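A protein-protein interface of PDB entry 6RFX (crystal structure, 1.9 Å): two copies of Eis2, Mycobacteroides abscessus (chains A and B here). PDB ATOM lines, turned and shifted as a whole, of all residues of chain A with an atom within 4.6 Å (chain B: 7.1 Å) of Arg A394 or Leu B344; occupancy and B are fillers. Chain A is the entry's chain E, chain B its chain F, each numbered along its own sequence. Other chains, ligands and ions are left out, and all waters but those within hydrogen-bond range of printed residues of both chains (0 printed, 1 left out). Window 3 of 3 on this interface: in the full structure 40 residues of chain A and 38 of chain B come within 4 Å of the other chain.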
ATOM      1  N   GLY A 390      32.326 -29.338   0.975  1.00  0.00           N
ATOM      2  CA  GLY A 390      31.035 -28.795   1.338  1.00  0.00           C
ATOM      3  C   GLY A 390      30.882 -27.303   1.159  1.00  0.00           C
ATOM      4  O   GLY A 390      29.766 -26.790   1.324  1.00  0.00           O
ATOM      5  N   ALA A 391      31.954 -26.584   0.819  1.00  0.00           N
ATOM      6  CA  ALA A 391      31.876 -25.129   0.743  1.00  0.00           C
ATOM      7  C   ALA A 391      31.031 -24.671  -0.441  1.00  0.00           C
ATOM      8  O   ALA A 391      30.245 -23.724  -0.317  1.00  0.00           O
ATOM      9  CB  ALA A 391      33.280 -24.530   0.673  1.00  0.00           C
ATOM     10  N   VAL A 392      31.180 -25.322  -1.595  1.00  0.00           N
ATOM     11  CA  VAL A 392      30.457 -24.886  -2.789  1.00  0.00           C
ATOM     12  C   VAL A 392      28.956 -25.081  -2.618  1.00  0.00           C
ATOM     13  O   VAL A 392      28.160 -24.208  -2.985  1.00  0.00           O
ATOM     14  CB  VAL A 392      31.002 -25.590  -4.045  1.00  0.00           C
ATOM     15  CG1 VAL A 392      30.105 -25.318  -5.242  1.00  0.00           C
ATOM     16  CG2 VAL A 392      32.414 -25.122  -4.334  1.00  0.00           C
ATOM     17  N   GLN A 393      28.551 -26.221  -2.048  1.00  0.00           N
ATOM     18  CA  GLN A 393      27.133 -26.527  -1.869  1.00  0.00           C
ATOM     19  C   GLN A 393      26.405 -25.397  -1.152  1.00  0.00           C
ATOM     20  O   GLN A 393      25.405 -24.868  -1.650  1.00  0.00           O
ATOM     21  CB  GLN A 393      26.995 -27.832  -1.080  1.00  0.00           C
ATOM     22  CG  GLN A 393      25.954 -28.806  -1.620  1.00  0.00           C
ATOM     23  CD  GLN A 393      24.525 -28.355  -1.376  1.00  0.00           C
ATOM     24  OE1 GLN A 393      24.271 -27.435  -0.597  1.00  0.00           O
ATOM     25  NE2 GLN A 393      23.580 -29.010  -2.040  1.00  0.00           N
ATOM     26  N   ARG A 394      26.906 -25.006   0.023  1.00  0.00           N
ATOM     27  CA  ARG A 394      26.231 -23.984   0.815  1.00  0.00           C
ATOM     28  C   ARG A 394      26.327 -22.611   0.161  1.00  0.00           C
ATOM     29  O   ARG A 394      25.348 -21.855   0.149  1.00  0.00           O
ATOM     30  CB  ARG A 394      26.802 -23.961   2.233  1.00  0.00           C
ATOM     31  CG  ARG A 394      26.365 -25.149   3.079  1.00  0.00           C
ATOM     32  CD  ARG A 394      27.372 -25.472   4.173  1.00  0.00           C
ATOM     33  NE  ARG A 394      26.961 -26.635   4.956  1.00  0.00           N
ATOM     34  CZ  ARG A 394      27.090 -27.896   4.551  1.00  0.00           C
ATOM     35  NH1 ARG A 394      27.615 -28.166   3.362  1.00  0.00           N
ATOM     36  NH2 ARG A 394      26.687 -28.888   5.331  1.00  0.00           N
ATOM     37  N   ALA A 395      27.493 -22.270  -0.390  1.00  0.00           N
ATOM     38  CA  ALA A 395      27.654 -20.961  -1.015  1.00  0.00           C
ATOM     39  C   ALA A 395      26.800 -20.820  -2.270  1.00  0.00           C
ATOM     40  O   ALA A 395      26.322 -19.720  -2.570  1.00  0.00           O
ATOM     41  CB  ALA A 395      29.126 -20.700  -1.332  1.00  0.00           C
ATOM     42  N   ALA A 396      26.594 -21.912  -3.011  1.00  0.00           N
ATOM     43  CA  ALA A 396      25.760 -21.843  -4.207  1.00  0.00           C
ATOM     44  C   ALA A 396      24.309 -21.546  -3.851  1.00  0.00           C
ATOM     45  O   ALA A 396      23.666 -20.712  -4.498  1.00  0.00           O
ATOM     46  CB  ALA A 396      25.865 -23.144  -5.002  1.00  0.00           C
ATOM     47  N   THR A 397      23.778 -22.219  -2.829  1.00  0.00           N
ATOM     48  CA  THR A 397      22.401 -21.968  -2.414  1.00  0.00           C
ATOM     49  C   THR A 397      22.237 -20.548  -1.883  1.00  0.00           C
ATOM     50  O   THR A 397      21.219 -19.893  -2.141  1.00  0.00           O
ATOM     51  CB  THR A 397      21.981 -22.995  -1.362  1.00  0.00           C
ATOM     52  OG1 THR A 397      22.083 -24.315  -1.912  1.00  0.00           O
ATOM     53  CG2 THR A 397      20.547 -22.749  -0.914  1.00  0.00           C
ATOM     54  N   ALA A 398      23.236 -20.051  -1.150  1.00  0.00           N
ATOM     55  CA  ALA A 398      23.151 -18.700  -0.605  1.00  0.00           C
ATOM     56  C   ALA A 398      23.169 -17.650  -1.709  1.00  0.00           C
ATOM     57  O   ALA A 398      22.415 -16.672  -1.652  1.00  0.00           O
ATOM     58  CB  ALA A 398      24.289 -18.462   0.384  1.00  0.00           C
ATOM     59  N   PRO B  70      17.370 -35.040  -5.197  1.00  0.00           N
ATOM     60  CA  PRO B  70      18.321 -34.036  -4.699  1.00  0.00           C
ATOM     61  C   PRO B  70      19.003 -34.482  -3.416  1.00  0.00           C
ATOM     62  O   PRO B  70      18.341 -34.771  -2.414  1.00  0.00           O
ATOM     63  CB  PRO B  70      17.435 -32.805  -4.468  1.00  0.00           C
ATOM     64  CG  PRO B  70      16.341 -32.958  -5.465  1.00  0.00           C
ATOM     65  CD  PRO B  70      16.073 -34.438  -5.556  1.00  0.00           C
ATOM     66  N   GLY B  71      20.336 -34.554  -3.445  1.00  0.00           N
ATOM     67  CA  GLY B  71      21.135 -35.055  -2.347  1.00  0.00           C
ATOM     68  C   GLY B  71      21.858 -36.348  -2.666  1.00  0.00           C
ATOM     69  O   GLY B  71      22.936 -36.598  -2.112  1.00  0.00           O
ATOM     70  N   ARG B 315      16.717 -34.519   0.172  1.00  0.00           N
ATOM     71  CA  ARG B 315      17.336 -33.510   1.019  1.00  0.00           C
ATOM     72  C   ARG B 315      17.069 -32.122   0.450  1.00  0.00           C
ATOM     73  O   ARG B 315      16.673 -31.962  -0.707  1.00  0.00           O
ATOM     74  CB  ARG B 315      18.842 -33.754   1.146  1.00  0.00           C
ATOM     75  CG  ARG B 315      19.195 -34.984   1.969  1.00  0.00           C
ATOM     76  CD  ARG B 315      18.655 -34.861   3.385  1.00  0.00           C
ATOM     77  NE  ARG B 315      18.876 -36.071   4.173  1.00  0.00           N
ATOM     78  CZ  ARG B 315      18.012 -37.079   4.247  1.00  0.00           C
ATOM     79  NH1 ARG B 315      16.869 -37.024   3.577  1.00  0.00           N
ATOM     80  NH2 ARG B 315      18.290 -38.143   4.988  1.00  0.00           N
ATOM     81  N   TYR B 316      17.293 -31.110   1.283  1.00  0.00           N
ATOM     82  CA  TYR B 316      16.921 -29.742   0.962  1.00  0.00           C
ATOM     83  C   TYR B 316      18.138 -28.831   1.044  1.00  0.00           C
ATOM     84  O   TYR B 316      18.967 -28.966   1.948  1.00  0.00           O
ATOM     85  CB  TYR B 316      15.794 -29.263   1.883  1.00  0.00           C
ATOM     86  CG  TYR B 316      14.542 -30.096   1.721  1.00  0.00           C
ATOM     87  CD1 TYR B 316      13.577 -29.751   0.785  1.00  0.00           C
ATOM     88  CD2 TYR B 316      14.341 -31.246   2.476  1.00  0.00           C
ATOM     89  CE1 TYR B 316      12.436 -30.515   0.617  1.00  0.00           C
ATOM     90  CE2 TYR B 316      13.202 -32.017   2.317  1.00  0.00           C
ATOM     91  CZ  TYR B 316      12.254 -31.646   1.385  1.00  0.00           C
ATOM     92  OH  TYR B 316      11.117 -32.402   1.213  1.00  0.00           O
ATOM     93  N   ALA B 317      18.234 -27.904   0.085  1.00  0.00           N
ATOM     94  CA  ALA B 317      19.431 -27.083  -0.066  1.00  0.00           C
ATOM     95  C   ALA B 317      19.697 -26.202   1.144  1.00  0.00           C
ATOM     96  O   ALA B 317      20.838 -25.771   1.343  1.00  0.00           O
ATOM     97  CB  ALA B 317      19.329 -26.232  -1.333  1.00  0.00           C
ATOM     98  N   ALA B 318      18.675 -25.915   1.946  1.00  0.00           N
ATOM     99  CA  ALA B 318      18.851 -25.196   3.197  1.00  0.00           C
ATOM    100  C   ALA B 318      17.744 -25.618   4.153  1.00  0.00           C
ATOM    101  O   ALA B 318      16.817 -26.341   3.780  1.00  0.00           O
ATOM    102  CB  ALA B 318      18.880 -23.679   2.982  1.00  0.00           C
ATOM    103  N   ASP B 319      17.854 -25.163   5.398  1.00  0.00           N
ATOM    104  CA  ASP B 319      16.923 -25.583   6.437  1.00  0.00           C
ATOM    105  C   ASP B 319      15.521 -25.054   6.164  1.00  0.00           C
ATOM    106  O   ASP B 319      15.343 -23.941   5.662  1.00  0.00           O
ATOM    107  CB  ASP B 319      17.406 -25.094   7.802  1.00  0.00           C
ATOM    108  CG  ASP B 319      18.498 -25.972   8.381  1.00  0.00           C
ATOM    109  OD1 ASP B 319      18.256 -27.186   8.557  1.00  0.00           O
ATOM    110  OD2 ASP B 319      19.601 -25.452   8.650  1.00  0.00           O
ATOM    111  N   GLY B 342      13.345 -30.164   6.954  1.00  0.00           N
ATOM    112  CA  GLY B 342      14.350 -30.652   6.036  1.00  0.00           C
ATOM    113  C   GLY B 342      15.603 -29.802   6.067  1.00  0.00           C
ATOM    114  O   GLY B 342      15.607 -28.664   6.543  1.00  0.00           O
ATOM    115  N   GLY B 343      16.671 -30.385   5.542  1.00  0.00           N
ATOM    116  CA  GLY B 343      17.944 -29.704   5.455  1.00  0.00           C
ATOM    117  C   GLY B 343      18.894 -30.483   4.574  1.00  0.00           C
ATOM    118  O   GLY B 343      18.497 -31.416   3.873  1.00  0.00           O
ATOM    119  N   LEU B 344      20.166 -30.086   4.618  1.00  0.00           N
ATOM    120  CA  LEU B 344      21.170 -30.773   3.813  1.00  0.00           C
ATOM    121  C   LEU B 344      21.397 -32.204   4.289  1.00  0.00           C
ATOM    122  O   LEU B 344      21.751 -33.072   3.483  1.00  0.00           O
ATOM    123  CB  LEU B 344      22.482 -29.990   3.813  1.00  0.00           C
ATOM    124  CG  LEU B 344      22.502 -28.676   3.028  1.00  0.00           C
ATOM    125  CD1 LEU B 344      23.840 -27.975   3.188  1.00  0.00           C
ATOM    126  CD2 LEU B 344      22.204 -28.927   1.559  1.00  0.00           C
ATOM    127  N   ASP B 345      21.183 -32.476   5.579  1.00  0.00           N
ATOM    128  CA  ASP B 345      21.498 -33.780   6.152  1.00  0.00           C
ATOM    129  C   ASP B 345      20.325 -34.438   6.872  1.00  0.00           C
ATOM    130  O   ASP B 345      20.535 -35.424   7.588  1.00  0.00           O
ATOM    131  CB  ASP B 345      22.705 -33.683   7.095  1.00  0.00           C
ATOM    132  CG  ASP B 345      22.470 -32.723   8.247  1.00  0.00           C
ATOM    133  OD1 ASP B 345      21.698 -31.757   8.067  1.00  0.00           O
ATOM    134  OD2 ASP B 345      23.058 -32.931   9.330  1.00  0.00           O
ATOM    135  N   HIS B 346      19.105 -33.934   6.704  1.00  0.00           N
ATOM    136  CA  HIS B 346      17.958 -34.509   7.395  1.00  0.00           C
ATOM    137  C   HIS B 346      16.691 -34.124   6.646  1.00  0.00           C
ATOM    138  O   HIS B 346      16.651 -33.117   5.935  1.00  0.00           O
ATOM    139  CB  HIS B 346      17.877 -34.039   8.853  1.00  0.00           C
ATOM    140  CG  HIS B 346      17.386 -32.633   9.007  1.00  0.00           C
ATOM    141  ND1 HIS B 346      18.217 -31.538   8.895  1.00  0.00           N
ATOM    142  CD2 HIS B 346      16.150 -32.141   9.262  1.00  0.00           C
ATOM    143  CE1 HIS B 346      17.515 -30.434   9.073  1.00  0.00           C
ATOM    144  NE2 HIS B 346      16.257 -30.772   9.298  1.00  0.00           N
ATOM    145  N   ALA B 347      15.655 -34.940   6.827  1.00  0.00           N
ATOM    146  CA  ALA B 347      14.365 -34.693   6.200  1.00  0.00           C
ATOM    147  C   ALA B 347      13.322 -35.561   6.886  1.00  0.00           C
ATOM    148  O   ALA B 347      13.526 -36.768   7.046  1.00  0.00           O
ATOM    149  CB  ALA B 347      14.419 -35.023   4.706  1.00  0.00           C
ATOM    150  N   TRP B 401      17.734 -26.673  -5.407  1.00  0.00           N
ATOM    151  CA  TRP B 401      18.951 -27.464  -5.309  1.00  0.00           C
ATOM    152  C   TRP B 401      20.013 -26.798  -6.166  1.00  0.00           C
ATOM    153  O   TRP B 401      19.672 -26.232  -7.213  1.00  0.00           O
ATOM    154  CB  TRP B 401      18.703 -28.901  -5.788  1.00  0.00           C
ATOM    155  CG  TRP B 401      19.765 -29.859  -5.358  1.00  0.00           C
ATOM    156  CD1 TRP B 401      20.655 -30.512  -6.158  1.00  0.00           C
ATOM    157  CD2 TRP B 401      20.064 -30.259  -4.013  1.00  0.00           C
ATOM    158  NE1 TRP B 401      21.485 -31.300  -5.398  1.00  0.00           N
ATOM    159  CE2 TRP B 401      21.144 -31.161  -4.078  1.00  0.00           C
ATOM    160  CE3 TRP B 401      19.523 -29.942  -2.763  1.00  0.00           C
ATOM    161  CZ2 TRP B 401      21.693 -31.748  -2.941  1.00  0.00           C
ATOM    162  CZ3 TRP B 401      20.068 -30.530  -1.636  1.00  0.00           C
ATOM    163  CH2 TRP B 401      21.141 -31.423  -1.731  1.00  0.00           C
ATOM    164  N   PRO B 402      21.286 -26.825  -5.763  1.00  0.00           N
ATOM    165  CA  PRO B 402      22.318 -26.136  -6.558  1.00  0.00           C
ATOM    166  C   PRO B 402      22.512 -26.714  -7.948  1.00  0.00           C
ATOM    167  O   PRO B 402      22.973 -25.991  -8.840  1.00  0.00           O
ATOM    168  CB  PRO B 402      23.584 -26.280  -5.703  1.00  0.00           C
ATOM    169  CG  PRO B 402      23.091 -26.580  -4.329  1.00  0.00           C
ATOM    170  CD  PRO B 402      21.833 -27.369  -4.510  1.00  0.00           C
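Arg A394 touches just one residue of chain B: Leu B344 (3.5 Å).
Printed residues of chain B within 4 Å of Ala A396: Pro B402.
Of the printed residues of chain B, Thr A397 touches Ala B317 and Pro B402.
Of the printed residues of chain A, Ala B317 touches Thr A397 (3.4 Å).
Leu B344 touches just these residues of chain A: Gln A393 (3.3 Å) and Arg A394 (3.5 Å).
Of the printed residues of chain A, Trp B401 touches Gln A393.
The nearest printed residue of chain A that does not touch Leu B344 is Thr A397 (5.8 Å).
The nearest printed residue of chain A that does not touch Trp B401 is Thr A397 (5.3 Å).
N of Leu B344 is in hydrogen-bond range of O of Tyr B316 (3.1 Å).
The guanidinium group of Arg A394 lies within hydrogen-bond range of the backbone carbonyl oxygen of Gly A390 (3.3 Å).
The backbone carbonyl oxygen (O) of Gln A393 sits at hydrogen-bond distance from the side-chain hydroxyl (OG1) of Thr A397.
Of the 9 printed residues of chain A, 4 touch a printed residue of chain B.
Printed residues of chain A that touch a printed residue of chain B: Gln A393, Arg A394, Ala A396 and Thr A397.
Hydrophobic or aromatic side chains of chain A within 4 Å of the printed part of chain B: Ala A396.
Of the 15 printed residues of chain B, 4 touch a printed residue of chain A.
Hydrophobic or aromatic side chains of chain B that line the printed part of chain A: Ala B317, Leu B344, Trp B401 and Pro B402.
Among the printed residues, 7 pairs touch across the chains.
No position is printed for both chains.
Among the printed residues, pairs that only touch across the chains: Gln A393 with Leu B344 (3.3 Å), Gln A393 with Pro B402 (3.4 Å), Thr A397 with Ala B317 (3.4 Å), Gln A393 with Trp B401 (3.4 Å), Thr A397 with Pro B402 (3.5 Å), Arg A394 with Leu B344 (3.5 Å) and Ala A396 with Pro B402 (3.9 Å).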
